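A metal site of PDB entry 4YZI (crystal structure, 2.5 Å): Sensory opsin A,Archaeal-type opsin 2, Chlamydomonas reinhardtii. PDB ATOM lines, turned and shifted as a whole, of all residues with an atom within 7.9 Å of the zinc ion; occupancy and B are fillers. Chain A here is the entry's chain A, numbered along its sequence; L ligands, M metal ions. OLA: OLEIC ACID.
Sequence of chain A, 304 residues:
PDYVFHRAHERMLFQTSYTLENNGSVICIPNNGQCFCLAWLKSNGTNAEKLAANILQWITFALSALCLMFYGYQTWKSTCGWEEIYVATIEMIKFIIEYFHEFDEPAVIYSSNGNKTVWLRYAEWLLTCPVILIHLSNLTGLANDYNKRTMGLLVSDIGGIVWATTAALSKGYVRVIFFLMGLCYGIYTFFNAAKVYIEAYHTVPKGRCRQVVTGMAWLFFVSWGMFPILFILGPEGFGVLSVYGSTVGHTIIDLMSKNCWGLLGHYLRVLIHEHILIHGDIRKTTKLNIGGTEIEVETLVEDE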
ATOM      1  N   PRO A   1     -24.626 -10.130  20.531  1.00  0.00           N
ATOM      2  CA  PRO A   1     -25.858 -10.866  20.200  1.00  0.00           C
ATOM      3  C   PRO A   1     -25.672 -11.757  18.987  1.00  0.00           C
ATOM      4  O   PRO A   1     -25.636 -11.266  17.861  1.00  0.00           O
ATOM      5  CB  PRO A   1     -26.851  -9.738  19.901  1.00  0.00           C
ATOM      6  CG  PRO A   1     -26.348  -8.575  20.672  1.00  0.00           C
ATOM      7  CD  PRO A   1     -24.853  -8.678  20.611  1.00  0.00           C
ATOM      8  N   ASP A   2     -25.561 -13.066  19.231  1.00  0.00           N
ATOM      9  CA  ASP A   2     -25.304 -14.034  18.169  1.00  0.00           C
ATOM     10  C   ASP A   2     -26.434 -14.068  17.141  1.00  0.00           C
ATOM     11  O   ASP A   2     -26.220 -14.407  15.970  1.00  0.00           O
ATOM     12  CB  ASP A   2     -25.088 -15.432  18.770  1.00  0.00           C
ATOM     13  CG  ASP A   2     -24.485 -16.411  17.772  1.00  0.00           C
ATOM     14  OD1 ASP A   2     -23.278 -16.294  17.485  1.00  0.00           O
ATOM     15  OD2 ASP A   2     -25.213 -17.303  17.280  1.00  0.00           O
ATOM     16  N   TYR A   3     -27.639 -13.728  17.574  1.00  0.00           N
ATOM     17  CA  TYR A   3     -28.802 -13.715  16.687  1.00  0.00           C
ATOM     18  C   TYR A   3     -28.646 -12.672  15.587  1.00  0.00           C
ATOM     19  O   TYR A   3     -29.243 -12.797  14.525  1.00  0.00           O
ATOM     20  CB  TYR A   3     -30.073 -13.452  17.501  1.00  0.00           C
ATOM     21  N   VAL A   4     -27.832 -11.657  15.852  1.00  0.00           N
ATOM     22  CA  VAL A   4     -27.633 -10.552  14.919  1.00  0.00           C
ATOM     23  C   VAL A   4     -26.241 -10.592  14.297  1.00  0.00           C
ATOM     24  O   VAL A   4     -26.070 -10.286  13.116  1.00  0.00           O
ATOM     25  CB  VAL A   4     -27.836  -9.188  15.633  1.00  0.00           C
ATOM     26  CG1 VAL A   4     -27.597  -8.037  14.665  1.00  0.00           C
ATOM     27  CG2 VAL A   4     -29.219  -9.108  16.239  1.00  0.00           C
ATOM     28  N   PHE A   5     -25.253 -10.998  15.079  1.00  0.00           N
ATOM     29  CA  PHE A   5     -23.848 -10.838  14.708  1.00  0.00           C
ATOM     30  C   PHE A   5     -23.148 -12.082  14.161  1.00  0.00           C
ATOM     31  O   PHE A   5     -21.992 -11.996  13.748  1.00  0.00           O
ATOM     32  CB  PHE A   5     -23.058 -10.318  15.907  1.00  0.00           C
ATOM     33  CG  PHE A   5     -23.183  -8.841  16.133  1.00  0.00           C
ATOM     34  CD1 PHE A   5     -24.376  -8.287  16.570  1.00  0.00           C
ATOM     35  CD2 PHE A   5     -22.107  -7.998  15.907  1.00  0.00           C
ATOM     36  CE1 PHE A   5     -24.488  -6.921  16.772  1.00  0.00           C
ATOM     37  CE2 PHE A   5     -22.207  -6.638  16.112  1.00  0.00           C
ATOM     38  CZ  PHE A   5     -23.404  -6.096  16.543  1.00  0.00           C
ATOM     39  N   HIS A   6     -23.817 -13.230  14.163  1.00  0.00           N
ATOM     40  CA  HIS A   6     -23.130 -14.466  13.785  1.00  0.00           C
ATOM     41  C   HIS A   6     -22.669 -14.482  12.323  1.00  0.00           C
ATOM     42  O   HIS A   6     -21.539 -14.882  12.041  1.00  0.00           O
ATOM     43  CB  HIS A   6     -23.990 -15.708  14.038  1.00  0.00           C
ATOM     44  CG  HIS A   6     -23.292 -16.995  13.715  1.00  0.00           C
ATOM     45  ND1 HIS A   6     -22.174 -17.417  14.398  1.00  0.00           N
ATOM     46  CD2 HIS A   6     -23.536 -17.930  12.772  1.00  0.00           C
ATOM     47  CE1 HIS A   6     -21.764 -18.570  13.897  1.00  0.00           C
ATOM     48  NE2 HIS A   6     -22.575 -18.897  12.909  1.00  0.00           N
ATOM     49  N   ARG A   7     -23.541 -14.068  11.410  1.00  0.00           N
ATOM     50  CA  ARG A   7     -23.190 -14.007   9.997  1.00  0.00           C
ATOM     51  C   ARG A   7     -21.977 -13.107   9.771  1.00  0.00           C
ATOM     52  O   ARG A   7     -21.201 -13.323   8.841  1.00  0.00           O
ATOM     53  CB  ARG A   7     -24.375 -13.518   9.161  1.00  0.00           C
ATOM     54  N   ALA A   8     -21.830 -12.110  10.638  1.00  0.00           N
ATOM     55  CA  ALA A   8     -20.724 -11.157  10.534  1.00  0.00           C
ATOM     56  C   ALA A   8     -19.403 -11.753  11.010  1.00  0.00           C
ATOM     57  O   ALA A   8     -18.396 -11.675  10.312  1.00  0.00           O
ATOM     58  CB  ALA A   8     -21.045  -9.898  11.308  1.00  0.00           C
ATOM     59  N   HIS A   9     -19.401 -12.341  12.209  1.00  0.00           N
ATOM     60  CA  HIS A   9     -18.147 -12.771  12.820  1.00  0.00           C
ATOM     61  C   HIS A   9     -17.824 -14.248  12.622  1.00  0.00           C
ATOM     62  O   HIS A   9     -16.833 -14.741  13.167  1.00  0.00           O
ATOM     63  CB  HIS A   9     -18.149 -12.439  14.321  1.00  0.00           C
ATOM     64  CG  HIS A   9     -19.203 -13.150  15.122  1.00  0.00           C
ATOM     65  ND1 HIS A   9     -19.719 -12.629  16.288  1.00  0.00           N
ATOM     66  CD2 HIS A   9     -19.821 -14.338  14.924  1.00  0.00           C
ATOM     67  CE1 HIS A   9     -20.619 -13.469  16.774  1.00  0.00           C
ATOM     68  NE2 HIS A   9     -20.695 -14.516  15.977  1.00  0.00           N
ATOM     69  N   GLU A  10     -18.640 -14.956  11.838  1.00  0.00           N
ATOM     70  CA  GLU A  10     -18.351 -16.370  11.579  1.00  0.00           C
ATOM     71  C   GLU A  10     -17.173 -16.482  10.632  1.00  0.00           C
ATOM     72  O   GLU A  10     -16.572 -17.546  10.488  1.00  0.00           O
ATOM     73  CB  GLU A  10     -19.585 -17.096  11.010  1.00  0.00           C
ATOM     74  CG  GLU A  10     -19.652 -17.177   9.492  1.00  0.00           C
ATOM     75  CD  GLU A  10     -20.299 -18.479   9.021  1.00  0.00           C
ATOM     76  OE1 GLU A  10     -21.061 -18.446   8.038  1.00  0.00           O
ATOM     77  OE2 GLU A  10     -20.029 -19.530   9.647  1.00  0.00           O
ATOM     78  N   LEU A  13     -14.420 -17.331  12.873  1.00  0.00           N
ATOM     79  CA  LEU A  13     -14.500 -18.656  13.477  1.00  0.00           C
ATOM     80  C   LEU A  13     -13.722 -19.684  12.663  1.00  0.00           C
ATOM     81  O   LEU A  13     -12.884 -20.414  13.192  1.00  0.00           O
ATOM     82  CB  LEU A  13     -15.955 -19.103  13.628  1.00  0.00           C
ATOM     83  CG  LEU A  13     -16.556 -18.991  15.031  1.00  0.00           C
ATOM     84  CD1 LEU A  13     -16.517 -17.554  15.543  1.00  0.00           C
ATOM     85  CD2 LEU A  13     -17.987 -19.522  15.035  1.00  0.00           C
ATOM     86  N   GLU A  98     -26.170 -18.870  25.038  1.00  0.00           N
ATOM     87  CA  GLU A  98     -26.882 -18.883  23.772  1.00  0.00           C
ATOM     88  C   GLU A  98     -26.939 -17.491  23.145  1.00  0.00           C
ATOM     89  O   GLU A  98     -26.703 -17.332  21.950  1.00  0.00           O
ATOM     90  CB  GLU A  98     -28.300 -19.420  23.952  1.00  0.00           C
ATOM     91  CG  GLU A  98     -28.444 -20.915  23.753  1.00  0.00           C
ATOM     92  CD  GLU A  98     -29.808 -21.436  24.146  1.00  0.00           C
ATOM     93  OE1 GLU A  98     -30.240 -22.466  23.581  1.00  0.00           O
ATOM     94  OE2 GLU A  98     -30.458 -20.817  25.025  1.00  0.00           O
ATOM     95  N   TYR A  99     -27.264 -16.508  23.977  1.00  0.00           N
ATOM     96  CA  TYR A  99     -27.466 -15.142  23.519  1.00  0.00           C
ATOM     97  C   TYR A  99     -26.249 -14.585  22.789  1.00  0.00           C
ATOM     98  O   TYR A  99     -26.380 -13.918  21.760  1.00  0.00           O
ATOM     99  CB  TYR A  99     -27.820 -14.239  24.711  1.00  0.00           C
ATOM    100  CG  TYR A  99     -28.026 -12.786  24.364  1.00  0.00           C
ATOM    101  CD1 TYR A  99     -29.273 -12.315  23.954  1.00  0.00           C
ATOM    102  CD2 TYR A  99     -26.986 -11.865  24.461  1.00  0.00           C
ATOM    103  CE1 TYR A  99     -29.473 -10.987  23.644  1.00  0.00           C
ATOM    104  CE2 TYR A  99     -27.173 -10.532  24.148  1.00  0.00           C
ATOM    105  CZ  TYR A  99     -28.416 -10.094  23.750  1.00  0.00           C
ATOM    106  OH  TYR A  99     -28.607  -8.764  23.445  1.00  0.00           O
ATOM    107  N   PHE A 100     -25.061 -14.871  23.310  1.00  0.00           N
ATOM    108  CA  PHE A 100     -23.826 -14.300  22.776  1.00  0.00           C
ATOM    109  C   PHE A 100     -23.090 -15.217  21.802  1.00  0.00           C
ATOM    110  O   PHE A 100     -22.521 -14.750  20.817  1.00  0.00           O
ATOM    111  CB  PHE A 100     -22.895 -13.908  23.919  1.00  0.00           C
ATOM    112  CG  PHE A 100     -23.384 -12.748  24.734  1.00  0.00           C
ATOM    113  CD1 PHE A 100     -23.365 -11.468  24.225  1.00  0.00           C
ATOM    114  CD2 PHE A 100     -23.858 -12.947  26.019  1.00  0.00           C
ATOM    115  CE1 PHE A 100     -23.810 -10.397  24.968  1.00  0.00           C
ATOM    116  CE2 PHE A 100     -24.311 -11.883  26.780  1.00  0.00           C
ATOM    117  CZ  PHE A 100     -24.293 -10.599  26.249  1.00  0.00           C
ATOM    118  N   HIS A 101     -23.088 -16.520  22.070  1.00  0.00           N
ATOM    119  CA  HIS A 101     -22.295 -17.443  21.255  1.00  0.00           C
ATOM    120  C   HIS A 101     -23.008 -18.758  20.935  1.00  0.00           C
ATOM    121  O   HIS A 101     -22.439 -19.826  21.155  1.00  0.00           O
ATOM    122  CB  HIS A 101     -20.973 -17.763  21.960  1.00  0.00           C
ATOM    123  CG  HIS A 101     -20.177 -16.559  22.344  1.00  0.00           C
ATOM    124  ND1 HIS A 101     -20.299 -15.965  23.591  1.00  0.00           N
ATOM    125  CD2 HIS A 101     -19.255 -15.839  21.673  1.00  0.00           C
ATOM    126  CE1 HIS A 101     -19.481 -14.923  23.660  1.00  0.00           C
ATOM    127  NE2 HIS A 101     -18.844 -14.824  22.500  1.00  0.00           N
ATOM    128  N   GLU A 102     -24.218 -18.688  20.405  1.00  0.00           N
ATOM    129  CA  GLU A 102     -24.996 -19.893  20.120  1.00  0.00           C
ATOM    130  C   GLU A 102     -24.336 -20.797  19.084  1.00  0.00           C
ATOM    131  O   GLU A 102     -24.301 -22.022  19.245  1.00  0.00           O
ATOM    132  CB  GLU A 102     -26.408 -19.537  19.667  1.00  0.00           C
ATOM    133  CG  GLU A 102     -27.189 -20.731  19.143  1.00  0.00           C
ATOM    134  CD  GLU A 102     -28.662 -20.691  19.523  1.00  0.00           C
ATOM    135  OE1 GLU A 102     -29.040 -19.839  20.353  1.00  0.00           O
ATOM    136  OE2 GLU A 102     -29.436 -21.517  18.989  1.00  0.00           O
ATOM    137  N   PHE A 103     -23.809 -20.211  18.020  1.00  0.00           N
ATOM    138  CA  PHE A 103     -23.234 -21.025  16.957  1.00  0.00           C
ATOM    139  C   PHE A 103     -21.717 -20.874  16.885  1.00  0.00           C
ATOM    140  O   PHE A 103     -21.102 -21.174  15.866  1.00  0.00           O
ATOM    141  CB  PHE A 103     -23.874 -20.675  15.615  1.00  0.00           C
ATOM    142  CG  PHE A 103     -25.357 -20.913  15.589  1.00  0.00           C
ATOM    143  CD1 PHE A 103     -25.858 -22.202  15.600  1.00  0.00           C
ATOM    144  CD2 PHE A 103     -26.243 -19.844  15.602  1.00  0.00           C
ATOM    145  CE1 PHE A 103     -27.213 -22.435  15.597  1.00  0.00           C
ATOM    146  CE2 PHE A 103     -27.610 -20.071  15.596  1.00  0.00           C
ATOM    147  CZ  PHE A 103     -28.087 -21.368  15.591  1.00  0.00           C
ATOM    148  N   ASP A 104     -21.138 -20.424  17.989  1.00  0.00           N
ATOM    149  CA  ASP A 104     -19.686 -20.314  18.103  1.00  0.00           C
ATOM    150  C   ASP A 104     -19.097 -21.532  18.805  1.00  0.00           C
ATOM    151  O   ASP A 104     -19.655 -22.026  19.785  1.00  0.00           O
ATOM    152  CB  ASP A 104     -19.313 -19.035  18.850  1.00  0.00           C
ATOM    153  CG  ASP A 104     -19.910 -17.789  18.213  1.00  0.00           C
ATOM    154  OD1 ASP A 104     -20.158 -17.816  16.993  1.00  0.00           O
ATOM    155  OD2 ASP A 104     -20.138 -16.799  18.928  1.00  0.00           O
ATOM    156  N   GLU A 105     -17.977 -22.012  18.284  1.00  0.00           N
ATOM    157  CA  GLU A 105     -17.247 -23.118  18.880  1.00  0.00           C
ATOM    158  C   GLU A 105     -16.815 -22.744  20.296  1.00  0.00           C
ATOM    159  O   GLU A 105     -16.304 -21.647  20.506  1.00  0.00           O
ATOM    160  CB  GLU A 105     -16.030 -23.459  18.015  1.00  0.00           C
ATOM    161  CG  GLU A 105     -15.416 -24.814  18.274  1.00  0.00           C
ATOM    162  CD  GLU A 105     -15.690 -25.781  17.145  1.00  0.00           C
ATOM    163  OE1 GLU A 105     -15.897 -25.323  16.006  1.00  0.00           O
ATOM    164  OE2 GLU A 105     -15.691 -27.006  17.394  1.00  0.00           O
ATOM    165  N   TYR A 110     -17.787 -27.785  15.274  1.00  0.00           N
ATOM    166  CA  TYR A 110     -17.599 -28.009  13.847  1.00  0.00           C
ATOM    167  C   TYR A 110     -16.413 -28.950  13.643  1.00  0.00           C
ATOM    168  O   TYR A 110     -15.264 -28.514  13.690  1.00  0.00           O
ATOM    169  CB  TYR A 110     -17.378 -26.687  13.095  1.00  0.00           C
ATOM    170  CG  TYR A 110     -18.506 -25.686  13.289  1.00  0.00           C
ATOM    171  CD1 TYR A 110     -18.559 -24.877  14.414  1.00  0.00           C
ATOM    172  CD2 TYR A 110     -19.497 -25.533  12.332  1.00  0.00           C
ATOM    173  CE1 TYR A 110     -19.571 -23.969  14.600  1.00  0.00           C
ATOM    174  CE2 TYR A 110     -20.529 -24.622  12.510  1.00  0.00           C
ATOM    175  CZ  TYR A 110     -20.550 -23.844  13.638  1.00  0.00           C
ATOM    176  OH  TYR A 110     -21.557 -22.925  13.830  1.00  0.00           O
HETATM  177  C1  OLA L   1     -16.079 -17.530  21.499  1.00  0.00           C
HETATM  178  O1  OLA L   1     -15.407 -16.476  21.418  1.00  0.00           O
HETATM  179  O2  OLA L   1     -16.223 -18.232  20.477  1.00  0.00           O
HETATM  180  C2  OLA L   1     -16.701 -17.936  22.806  1.00  0.00           C
HETATM  181  C3  OLA L   1     -16.855 -19.447  22.895  1.00  0.00           C
HETATM  182  C4  OLA L   1     -18.222 -19.796  23.477  1.00  0.00           C
HETATM  183  C5  OLA L   1     -18.151 -20.939  24.500  1.00  0.00           C
HETATM  184  C6  OLA L   1     -19.530 -21.549  24.693  1.00  0.00           C
HETATM  185  C7  OLA L   1     -19.447 -23.051  24.969  1.00  0.00           C
HETATM  186  C8  OLA L   1     -20.568 -23.467  25.919  1.00  0.00           C
HETATM  187  C9  OLA L   1     -20.514 -24.955  26.176  1.00  0.00           C
HETATM  188  C10 OLA L   1     -21.408 -25.529  27.189  1.00  0.00           C
HETATM  189  C11 OLA L   1     -21.704 -24.736  28.445  1.00  0.00           C
HETATM  190  C12 OLA L   1     -22.774 -25.456  29.259  1.00  0.00           C
HETATM  191 ZN    ZN M   1     -21.609 -16.480  16.331  1.00  0.00          ZN
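The backbone carbonyl oxygen of Tyr 99 lies within hydrogen-bond range of the backbone NH of Asp 2. The side-chain carboxylate of Asp 2 lies close to the backbone NH of Phe 103. ND1 of His 9 lies close to O of Phe 5 (3.5 Å).
Within 4 Å of the zinc ion: Asp 2, His 6, His 9 and Asp 104.
The zinc ion is bound by OD1 of Asp 2 (2.0 Å), OD1 of Asp 104 (2.1 Å), NE2 of His 9 (2.2 Å) and ND1 of His 6 (2.2 Å).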
